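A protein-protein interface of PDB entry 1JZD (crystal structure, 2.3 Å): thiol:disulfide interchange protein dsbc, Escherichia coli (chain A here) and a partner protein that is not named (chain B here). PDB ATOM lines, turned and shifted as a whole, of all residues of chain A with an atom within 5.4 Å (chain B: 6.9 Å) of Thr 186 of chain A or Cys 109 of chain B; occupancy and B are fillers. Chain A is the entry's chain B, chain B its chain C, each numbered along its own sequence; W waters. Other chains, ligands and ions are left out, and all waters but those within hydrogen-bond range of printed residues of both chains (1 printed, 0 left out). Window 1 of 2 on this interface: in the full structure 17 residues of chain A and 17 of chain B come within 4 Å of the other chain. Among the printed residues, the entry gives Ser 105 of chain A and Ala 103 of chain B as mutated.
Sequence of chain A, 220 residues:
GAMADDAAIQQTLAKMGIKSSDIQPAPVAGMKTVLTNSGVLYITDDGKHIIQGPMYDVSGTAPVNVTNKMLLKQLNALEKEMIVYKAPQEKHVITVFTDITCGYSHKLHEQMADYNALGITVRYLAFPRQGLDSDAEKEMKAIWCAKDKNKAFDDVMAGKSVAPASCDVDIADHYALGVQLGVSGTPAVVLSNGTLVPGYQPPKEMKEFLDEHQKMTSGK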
ATOM      1  N   PHE A  97      21.621 -12.829 -30.305  1.00  0.00           N
ATOM      2  CA  PHE A  97      22.132 -12.040 -31.413  1.00  0.00           C
ATOM      3  C   PHE A  97      23.451 -11.524 -30.892  1.00  0.00           C
ATOM      4  O   PHE A  97      23.487 -10.761 -29.932  1.00  0.00           O
ATOM      5  CB  PHE A  97      21.211 -10.879 -31.745  1.00  0.00           C
ATOM      6  CG  PHE A  97      19.969 -11.298 -32.459  1.00  0.00           C
ATOM      7  CD1 PHE A  97      18.855 -11.743 -31.750  1.00  0.00           C
ATOM      8  CD2 PHE A  97      19.943 -11.338 -33.844  1.00  0.00           C
ATOM      9  CE1 PHE A  97      17.733 -12.230 -32.413  1.00  0.00           C
ATOM     10  CE2 PHE A  97      18.819 -11.827 -34.524  1.00  0.00           C
ATOM     11  CZ  PHE A  97      17.715 -12.274 -33.808  1.00  0.00           C
ATOM     12  N   THR A  98      24.539 -11.954 -31.520  1.00  0.00           N
ATOM     13  CA  THR A  98      25.864 -11.570 -31.084  1.00  0.00           C
ATOM     14  C   THR A  98      26.651 -10.759 -32.122  1.00  0.00           C
ATOM     15  O   THR A  98      26.348 -10.777 -33.314  1.00  0.00           O
ATOM     16  CB  THR A  98      26.658 -12.833 -30.683  1.00  0.00           C
ATOM     17  OG1 THR A  98      27.874 -12.453 -30.029  1.00  0.00           O
ATOM     18  CG2 THR A  98      26.980 -13.674 -31.911  1.00  0.00           C
ATOM     19  N   ASP A  99      27.662 -10.045 -31.641  1.00  0.00           N
ATOM     20  CA  ASP A  99      28.508  -9.202 -32.469  1.00  0.00           C
ATOM     21  C   ASP A  99      29.926  -9.459 -31.978  1.00  0.00           C
ATOM     22  O   ASP A  99      30.192  -9.296 -30.791  1.00  0.00           O
ATOM     23  CB  ASP A  99      28.132  -7.735 -32.238  1.00  0.00           C
ATOM     24  CG  ASP A  99      28.914  -6.769 -33.120  1.00  0.00           C
ATOM     25  OD1 ASP A  99      30.010  -7.112 -33.616  1.00  0.00           O
ATOM     26  OD2 ASP A  99      28.425  -5.635 -33.299  1.00  0.00           O
ATOM     27  N   CYS A 102      31.938  -6.682 -30.001  1.00  0.00           N
ATOM     28  CA  CYS A 102      31.240  -6.235 -28.798  1.00  0.00           C
ATOM     29  C   CYS A 102      31.852  -6.939 -27.594  1.00  0.00           C
ATOM     30  O   CYS A 102      31.730  -8.153 -27.448  1.00  0.00           O
ATOM     31  CB  CYS A 102      29.750  -6.582 -28.914  1.00  0.00           C
ATOM     32  SG  CYS A 102      28.765  -6.467 -27.384  1.00  0.00           S
ATOM     33  N   GLY A 103      32.516  -6.171 -26.738  1.00  0.00           N
ATOM     34  CA  GLY A 103      33.149  -6.744 -25.568  1.00  0.00           C
ATOM     35  C   GLY A 103      32.233  -7.618 -24.731  1.00  0.00           C
ATOM     36  O   GLY A 103      32.679  -8.588 -24.138  1.00  0.00           O
ATOM     37  N   TYR A 104      30.947  -7.295 -24.688  1.00  0.00           N
ATOM     38  CA  TYR A 104      30.038  -8.088 -23.883  1.00  0.00           C
ATOM     39  C   TYR A 104      29.644  -9.399 -24.538  1.00  0.00           C
ATOM     40  O   TYR A 104      29.301 -10.341 -23.839  1.00  0.00           O
ATOM     41  CB  TYR A 104      28.801  -7.270 -23.512  1.00  0.00           C
ATOM     42  CG  TYR A 104      29.133  -6.180 -22.521  1.00  0.00           C
ATOM     43  CD1 TYR A 104      29.630  -6.492 -21.248  1.00  0.00           C
ATOM     44  CD2 TYR A 104      29.027  -4.838 -22.877  1.00  0.00           C
ATOM     45  CE1 TYR A 104      30.022  -5.494 -20.360  1.00  0.00           C
ATOM     46  CE2 TYR A 104      29.417  -3.834 -22.007  1.00  0.00           C
ATOM     47  CZ  TYR A 104      29.918  -4.159 -20.750  1.00  0.00           C
ATOM     48  OH  TYR A 104      30.345  -3.143 -19.920  1.00  0.00           O
ATOM     49  N   SER A 105      29.674  -9.449 -25.871  1.00  0.00           N
ATOM     50  CA  SER A 105      29.352 -10.677 -26.607  1.00  0.00           C
ATOM     51  C   SER A 105      30.501 -11.638 -26.300  1.00  0.00           C
ATOM     52  O   SER A 105      30.307 -12.852 -26.173  1.00  0.00           O
ATOM     53  CB  SER A 105      29.279 -10.404 -28.123  1.00  0.00           C
ATOM     54  OG  SER A 105      28.031  -9.812 -28.492  1.00  0.00           O
ATOM     55  N   PHE A 127      24.619 -10.254 -35.538  1.00  0.00           N
ATOM     56  CA  PHE A 127      23.995  -8.936 -35.492  1.00  0.00           C
ATOM     57  C   PHE A 127      25.068  -7.881 -35.323  1.00  0.00           C
ATOM     58  O   PHE A 127      25.339  -7.420 -34.209  1.00  0.00           O
ATOM     59  CB  PHE A 127      22.993  -8.806 -34.347  1.00  0.00           C
ATOM     60  CG  PHE A 127      22.108  -7.593 -34.468  1.00  0.00           C
ATOM     61  CD1 PHE A 127      20.862  -7.682 -35.089  1.00  0.00           C
ATOM     62  CD2 PHE A 127      22.551  -6.349 -34.034  1.00  0.00           C
ATOM     63  CE1 PHE A 127      20.072  -6.546 -35.279  1.00  0.00           C
ATOM     64  CE2 PHE A 127      21.775  -5.209 -34.217  1.00  0.00           C
ATOM     65  CZ  PHE A 127      20.531  -5.306 -34.843  1.00  0.00           C
ATOM     66  N   ARG A 129      26.195  -4.677 -34.837  1.00  0.00           N
ATOM     67  CA  ARG A 129      25.601  -3.407 -34.434  1.00  0.00           C
ATOM     68  C   ARG A 129      26.109  -2.256 -35.288  1.00  0.00           C
ATOM     69  O   ARG A 129      25.442  -1.225 -35.417  1.00  0.00           O
ATOM     70  CB  ARG A 129      25.883  -3.127 -32.948  1.00  0.00           C
ATOM     71  CG  ARG A 129      27.341  -2.813 -32.619  1.00  0.00           C
ATOM     72  CD  ARG A 129      27.529  -2.561 -31.128  1.00  0.00           C
ATOM     73  NE  ARG A 129      28.892  -2.147 -30.795  1.00  0.00           N
ATOM     74  CZ  ARG A 129      29.985  -2.824 -31.140  1.00  0.00           C
ATOM     75  NH1 ARG A 129      29.877  -3.944 -31.836  1.00  0.00           N
ATOM     76  NH2 ARG A 129      31.191  -2.392 -30.785  1.00  0.00           N
ATOM     77  N   VAL A 183      15.773  -5.530 -31.841  1.00  0.00           N
ATOM     78  CA  VAL A 183      17.168  -5.505 -31.426  1.00  0.00           C
ATOM     79  C   VAL A 183      17.852  -4.230 -31.914  1.00  0.00           C
ATOM     80  O   VAL A 183      17.765  -3.884 -33.094  1.00  0.00           O
ATOM     81  CB  VAL A 183      17.943  -6.712 -31.989  1.00  0.00           C
ATOM     82  CG1 VAL A 183      19.414  -6.661 -31.528  1.00  0.00           C
ATOM     83  CG2 VAL A 183      17.274  -8.001 -31.544  1.00  0.00           C
ATOM     84  N   SER A 184      18.526  -3.533 -31.007  1.00  0.00           N
ATOM     85  CA  SER A 184      19.226  -2.310 -31.364  1.00  0.00           C
ATOM     86  C   SER A 184      20.673  -2.424 -30.911  1.00  0.00           C
ATOM     87  O   SER A 184      21.585  -1.953 -31.583  1.00  0.00           O
ATOM     88  CB  SER A 184      18.555  -1.090 -30.718  1.00  0.00           C
ATOM     89  OG  SER A 184      18.488  -1.223 -29.305  1.00  0.00           O
ATOM     90  N   GLY A 185      20.886  -3.070 -29.776  1.00  0.00           N
ATOM     91  CA  GLY A 185      22.239  -3.232 -29.287  1.00  0.00           C
ATOM     92  C   GLY A 185      22.579  -4.694 -29.109  1.00  0.00           C
ATOM     93  O   GLY A 185      21.726  -5.562 -29.278  1.00  0.00           O
ATOM     94  N   THR A 186      23.827  -4.969 -28.765  1.00  0.00           N
ATOM     95  CA  THR A 186      24.265  -6.334 -28.567  1.00  0.00           C
ATOM     96  C   THR A 186      24.913  -6.497 -27.197  1.00  0.00           C
ATOM     97  O   THR A 186      25.453  -5.545 -26.644  1.00  0.00           O
ATOM     98  CB  THR A 186      25.255  -6.748 -29.676  1.00  0.00           C
ATOM     99  OG1 THR A 186      26.302  -5.778 -29.778  1.00  0.00           O
ATOM    100  CG2 THR A 186      24.542  -6.828 -31.012  1.00  0.00           C
ATOM    101  N   PRO A 187      24.829  -7.705 -26.616  1.00  0.00           N
ATOM    102  CA  PRO A 187      24.157  -8.867 -27.202  1.00  0.00           C
ATOM    103  C   PRO A 187      22.698  -8.792 -26.807  1.00  0.00           C
ATOM    104  O   PRO A 187      22.358  -8.103 -25.861  1.00  0.00           O
ATOM    105  CB  PRO A 187      24.867 -10.033 -26.539  1.00  0.00           C
ATOM    106  CG  PRO A 187      25.036  -9.510 -25.126  1.00  0.00           C
ATOM    107  CD  PRO A 187      25.503  -8.072 -25.356  1.00  0.00           C
ATOM    108  N   ALA A 188      21.835  -9.492 -27.526  1.00  0.00           N
ATOM    109  CA  ALA A 188      20.412  -9.475 -27.215  1.00  0.00           C
ATOM    110  C   ALA A 188      19.909 -10.910 -27.162  1.00  0.00           C
ATOM    111  O   ALA A 188      20.200 -11.726 -28.050  1.00  0.00           O
ATOM    112  CB  ALA A 188      19.643  -8.681 -28.273  1.00  0.00           C
ATOM    113  N   TYR B  40      28.804   4.635 -20.601  1.00  0.00           N
ATOM    114  CA  TYR B  40      30.086   5.257 -20.880  1.00  0.00           C
ATOM    115  C   TYR B  40      30.366   5.301 -22.383  1.00  0.00           C
ATOM    116  O   TYR B  40      29.771   4.562 -23.168  1.00  0.00           O
ATOM    117  CB  TYR B  40      31.198   4.495 -20.151  1.00  0.00           C
ATOM    118  CG  TYR B  40      31.223   3.007 -20.439  1.00  0.00           C
ATOM    119  CD1 TYR B  40      31.977   2.485 -21.495  1.00  0.00           C
ATOM    120  CD2 TYR B  40      30.480   2.119 -19.657  1.00  0.00           C
ATOM    121  CE1 TYR B  40      31.992   1.112 -21.756  1.00  0.00           C
ATOM    122  CE2 TYR B  40      30.484   0.759 -19.913  1.00  0.00           C
ATOM    123  CZ  TYR B  40      31.237   0.263 -20.954  1.00  0.00           C
ATOM    124  OH  TYR B  40      31.229  -1.089 -21.189  1.00  0.00           O
ATOM    125  N   TYR B  42      33.516   5.423 -25.405  1.00  0.00           N
ATOM    126  CA  TYR B  42      34.895   5.063 -25.655  1.00  0.00           C
ATOM    127  C   TYR B  42      35.607   6.252 -26.241  1.00  0.00           C
ATOM    128  O   TYR B  42      35.187   6.802 -27.257  1.00  0.00           O
ATOM    129  CB  TYR B  42      34.986   3.901 -26.639  1.00  0.00           C
ATOM    130  CG  TYR B  42      34.432   2.619 -26.100  1.00  0.00           C
ATOM    131  CD1 TYR B  42      33.097   2.278 -26.296  1.00  0.00           C
ATOM    132  CD2 TYR B  42      35.239   1.749 -25.367  1.00  0.00           C
ATOM    133  CE1 TYR B  42      32.579   1.098 -25.776  1.00  0.00           C
ATOM    134  CE2 TYR B  42      34.726   0.569 -24.843  1.00  0.00           C
ATOM    135  CZ  TYR B  42      33.404   0.250 -25.052  1.00  0.00           C
ATOM    136  OH  TYR B  42      32.909  -0.936 -24.562  1.00  0.00           O
ATOM    137  N   ASP B  68      37.887  -4.045 -22.112  1.00  0.00           N
ATOM    138  CA  ASP B  68      36.840  -4.896 -22.656  1.00  0.00           C
ATOM    139  C   ASP B  68      37.469  -5.896 -23.612  1.00  0.00           C
ATOM    140  O   ASP B  68      38.503  -5.636 -24.234  1.00  0.00           O
ATOM    141  CB  ASP B  68      35.721  -4.092 -23.344  1.00  0.00           C
ATOM    142  CG  ASP B  68      36.148  -3.492 -24.655  1.00  0.00           C
ATOM    143  OD1 ASP B  68      37.003  -2.579 -24.628  1.00  0.00           O
ATOM    144  OD2 ASP B  68      35.626  -3.934 -25.708  1.00  0.00           O
ATOM    145  N   TYR B  71      38.241  -4.156 -27.781  1.00  0.00           N
ATOM    146  CA  TYR B  71      39.145  -3.014 -27.909  1.00  0.00           C
ATOM    147  C   TYR B  71      40.318  -3.104 -26.933  1.00  0.00           C
ATOM    148  O   TYR B  71      41.294  -2.355 -27.058  1.00  0.00           O
ATOM    149  CB  TYR B  71      38.376  -1.699 -27.687  1.00  0.00           C
ATOM    150  CG  TYR B  71      37.238  -1.496 -28.669  1.00  0.00           C
ATOM    151  CD1 TYR B  71      35.923  -1.355 -28.226  1.00  0.00           C
ATOM    152  CD2 TYR B  71      37.475  -1.483 -30.045  1.00  0.00           C
ATOM    153  CE1 TYR B  71      34.868  -1.214 -29.128  1.00  0.00           C
ATOM    154  CE2 TYR B  71      36.433  -1.343 -30.951  1.00  0.00           C
ATOM    155  CZ  TYR B  71      35.132  -1.210 -30.488  1.00  0.00           C
ATOM    156  OH  TYR B  71      34.101  -1.085 -31.391  1.00  0.00           O
ATOM    157  N   GLN B 101      30.627   6.124 -29.955  1.00  0.00           N
ATOM    158  CA  GLN B 101      30.086   4.855 -29.552  1.00  0.00           C
ATOM    159  C   GLN B 101      30.195   4.709 -28.055  1.00  0.00           C
ATOM    160  O   GLN B 101      31.187   5.098 -27.440  1.00  0.00           O
ATOM    161  CB  GLN B 101      30.834   3.716 -30.232  1.00  0.00           C
ATOM    162  CG  GLN B 101      30.182   2.379 -29.991  1.00  0.00           C
ATOM    163  CD  GLN B 101      30.997   1.229 -30.540  1.00  0.00           C
ATOM    164  OE1 GLN B 101      31.013   0.139 -29.956  1.00  0.00           O
ATOM    165  NE2 GLN B 101      31.680   1.460 -31.672  1.00  0.00           N
ATOM    166  N   GLY B 102      29.150   4.149 -27.473  1.00  0.00           N
ATOM    167  CA  GLY B 102      29.119   3.964 -26.045  1.00  0.00           C
ATOM    168  C   GLY B 102      28.518   2.622 -25.694  1.00  0.00           C
ATOM    169  O   GLY B 102      28.093   1.863 -26.563  1.00  0.00           O
ATOM    170  N   ALA B 103      28.461   2.344 -24.405  1.00  0.00           N
ATOM    171  CA  ALA B 103      27.945   1.072 -23.946  1.00  0.00           C
ATOM    172  C   ALA B 103      27.401   1.221 -22.533  1.00  0.00           C
ATOM    173  O   ALA B 103      27.443   2.312 -21.969  1.00  0.00           O
ATOM    174  CB  ALA B 103      29.066   0.045 -23.986  1.00  0.00           C
ATOM    175  N   ALA B 104      26.888   0.129 -21.970  1.00  0.00           N
ATOM    176  CA  ALA B 104      26.341   0.155 -20.614  1.00  0.00           C
ATOM    177  C   ALA B 104      26.924  -0.965 -19.747  1.00  0.00           C
ATOM    178  O   ALA B 104      27.036  -2.110 -20.185  1.00  0.00           O
ATOM    179  CB  ALA B 104      24.829   0.047 -20.660  1.00  0.00           C
ATOM    180  N   GLY B 107      26.038  -4.639 -19.352  1.00  0.00           N
ATOM    181  CA  GLY B 107      26.293  -5.559 -20.450  1.00  0.00           C
ATOM    182  C   GLY B 107      25.567  -5.293 -21.751  1.00  0.00           C
ATOM    183  O   GLY B 107      24.789  -6.121 -22.215  1.00  0.00           O
ATOM    184  N   PHE B 108      25.846  -4.152 -22.367  1.00  0.00           N
ATOM    185  CA  PHE B 108      25.162  -3.796 -23.600  1.00  0.00           C
ATOM    186  C   PHE B 108      26.005  -2.825 -24.411  1.00  0.00           C
ATOM    187  O   PHE B 108      26.539  -1.860 -23.859  1.00  0.00           O
ATOM    188  CB  PHE B 108      23.828  -3.143 -23.231  1.00  0.00           C
ATOM    189  CG  PHE B 108      22.854  -3.037 -24.361  1.00  0.00           C
ATOM    190  CD1 PHE B 108      22.404  -4.178 -25.024  1.00  0.00           C
ATOM    191  CD2 PHE B 108      22.319  -1.802 -24.714  1.00  0.00           C
ATOM    192  CE1 PHE B 108      21.424  -4.093 -26.019  1.00  0.00           C
ATOM    193  CE2 PHE B 108      21.341  -1.703 -25.708  1.00  0.00           C
ATOM    194  CZ  PHE B 108      20.889  -2.855 -26.360  1.00  0.00           C
ATOM    195  N   CYS B 109      26.159  -3.101 -25.704  1.00  0.00           N
ATOM    196  CA  CYS B 109      26.897  -2.195 -26.585  1.00  0.00           C
ATOM    197  C   CYS B 109      25.915  -1.613 -27.569  1.00  0.00           C
ATOM    198  O   CYS B 109      25.113  -2.328 -28.167  1.00  0.00           O
ATOM    199  CB  CYS B 109      27.988  -2.887 -27.394  1.00  0.00           C
ATOM    200  SG  CYS B 109      29.233  -3.791 -26.441  1.00  0.00           S
ATOM    201  N   TYR B 110      25.983  -0.307 -27.735  1.00  0.00           N
ATOM    202  CA  TYR B 110      25.106   0.384 -28.657  1.00  0.00           C
ATOM    203  C   TYR B 110      25.800   0.549 -29.994  1.00  0.00           C
ATOM    204  O   TYR B 110      27.022   0.458 -30.087  1.00  0.00           O
ATOM    205  CB  TYR B 110      24.785   1.783 -28.155  1.00  0.00           C
ATOM    206  CG  TYR B 110      23.857   1.849 -26.983  1.00  0.00           C
ATOM    207  CD1 TYR B 110      24.325   1.683 -25.676  1.00  0.00           C
ATOM    208  CD2 TYR B 110      22.504   2.101 -27.175  1.00  0.00           C
ATOM    209  CE1 TYR B 110      23.461   1.774 -24.597  1.00  0.00           C
ATOM    210  CE2 TYR B 110      21.634   2.191 -26.104  1.00  0.00           C
ATOM    211  CZ  TYR B 110      22.112   2.027 -24.820  1.00  0.00           C
ATOM    212  OH  TYR B 110      21.222   2.105 -23.772  1.00  0.00           O
ATOM    213  N   PRO B 111      25.016   0.786 -31.050  1.00  0.00           N
ATOM    214  CA  PRO B 111      25.559   0.989 -32.398  1.00  0.00           C
ATOM    215  C   PRO B 111      26.197   2.387 -32.395  1.00  0.00           C
ATOM    216  O   PRO B 111      25.892   3.198 -31.533  1.00  0.00           O
ATOM    217  CB  PRO B 111      24.316   0.963 -33.281  1.00  0.00           C
ATOM    218  CG  PRO B 111      23.322   0.137 -32.478  1.00  0.00           C
ATOM    219  CD  PRO B 111      23.551   0.619 -31.078  1.00  0.00           C
HETATM  220  O   HOH W   1      33.327  -3.724 -27.510  1.00  0.00           O
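The backbone carbonyl oxygen of Ala 104 of chain B lies close to the side-chain hydroxyl of Tyr 104 of chain A (3.5 Å).
The side-chain hydroxyl (OH) of Tyr 104 of chain A is in hydrogen-bond range of the side-chain hydroxyl (OH) of Tyr 40 of chain B (2.6 Å).
The side-chain sulfur (SG) of Cys 102 of chain A sits close to the side-chain sulfur (SG) of Cys 109 of chain B (2.9 Å).
The side-chain amide oxygen (OE1) of Gln 101 of chain B sits at hydrogen-bond distance from the guanidinium group (NH2) of Arg 129 of chain A, at 2.7 Å.
The guanidinium group (NH2) of Arg 129 of chain A lies within hydrogen-bond range of the side-chain hydroxyl (OH) of Tyr 71 of chain B (3.2 Å).
N of Cys 109 of chain B lies within hydrogen-bond range of O of Thr 186 of chain A.
The guanidinium group (NE) of Arg 129 of chain A sits close to the backbone carbonyl oxygen (O) of Tyr 110 of chain B, 3.3 Å away.
The side-chain carboxylate (OD2) of Asp 68 of chain B is in hydrogen-bond range of the backbone NH (N) of Tyr 71 of chain B (3.3 Å).
O of Tyr 40 of chain B lies within hydrogen-bond range of N of Ala 103 of chain B.
The backbone NH (N) of Tyr 110 of chain B lies within hydrogen-bond range of the backbone carbonyl oxygen (O) of Gly 102 of chain B, at 3.2 Å.
The backbone NH (N) of Ser 105 of chain A is in hydrogen-bond range of the side-chain sulfur (SG) of Cys 102 of chain A (3.5 Å).
NH1 of Arg 129 of chain A is in salt-bridge range of OD2 of Asp 99 of chain A.
The side-chain sulfur (SG) of Cys 102 of chain A lies within hydrogen-bond range of the side-chain hydroxyl (OG1) of Thr 186 of chain A (3.5 Å).
Asp 68 of chain B touches Gly 103 of chain A (OD2 to CA, 3.7 Å).
CD2 of Tyr 104 of chain A touches N of Phe 108 of chain B, 3.3 Å away.
CD2 of Tyr 104 of chain A touches SG of Cys 109 of chain B, 3.7 Å away.
NE of Arg 129 of chain A touches CB of Cys 109 of chain B, at 3.6 Å.
Arg 129 of chain A touches Pro 111 of chain B (O to CB, 3.3 Å).
Pro 111 of chain B touches Ser 184 of chain A (CG to O, 2.9 Å).
CA of Gly 185 of chain A touches CZ of Phe 108 of chain B, at 3.2 Å.
Gly 185 of chain A touches Cys 109 of chain B (CA to O, 3.2 Å).
Thr 186 of chain A touches Phe 108 of chain B (O to CA, 3.5 Å).
O of Gly 107 of chain B touches CD of Pro 187 of chain A, at 3.8 Å.
Phe 97 of chain A touches none of the printed residues of chain B.
Printed residues of chain B within 4 Å of Gly 103 of chain A: Asp 68.
Of the printed residues of chain B, Arg 129 of chain A touches Tyr 71, Gln 101, Cys 109, Tyr 110 and Pro 111.
Thr 186 of chain A touches just these residues of chain B: Phe 108 and Cys 109.
Of the printed residues of chain B, Pro 187 of chain A touches Gly 107.
Of chain A, only Cys 102 (2.9 Å), Tyr 104 (3.7 Å), Arg 129 (3.6 Å), Gly 185 (3.2 Å) and Thr 186 (2.7 Å) come within 4 Å of Cys 109 of chain B.
Of the printed residues of chain A, Pro 111 of chain B touches Arg 129 and Ser 184.
The nearest residue of chain A that does not touch Cys 109 of chain B is Gly 103 of chain A (4.1 Å).
Of the 15 printed residues of chain A, 8 touch a printed residue of chain B.
Printed residues of chain A that touch a printed residue of chain B: Cys 102, Gly 103, Tyr 104, Arg 129, Ser 184, Gly 185, Thr 186 and Pro 187.
Printed residues of chain B that touch a printed residue of chain A: Tyr 40, Asp 68, Tyr 71, Gln 101, Ala 104, Gly 107, Phe 108, Cys 109, Tyr 110 and Pro 111.
Hydrophobic or aromatic side chains of chain B within 4 Å of the printed part of chain A: Tyr 40, Tyr 71, Phe 108 and Pro 111.
Water W1 lies within hydrogen-bond range of N of Gly 103 of chain A (2.7 Å) and OD2 of Asp 68 of chain B (2.9 Å).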
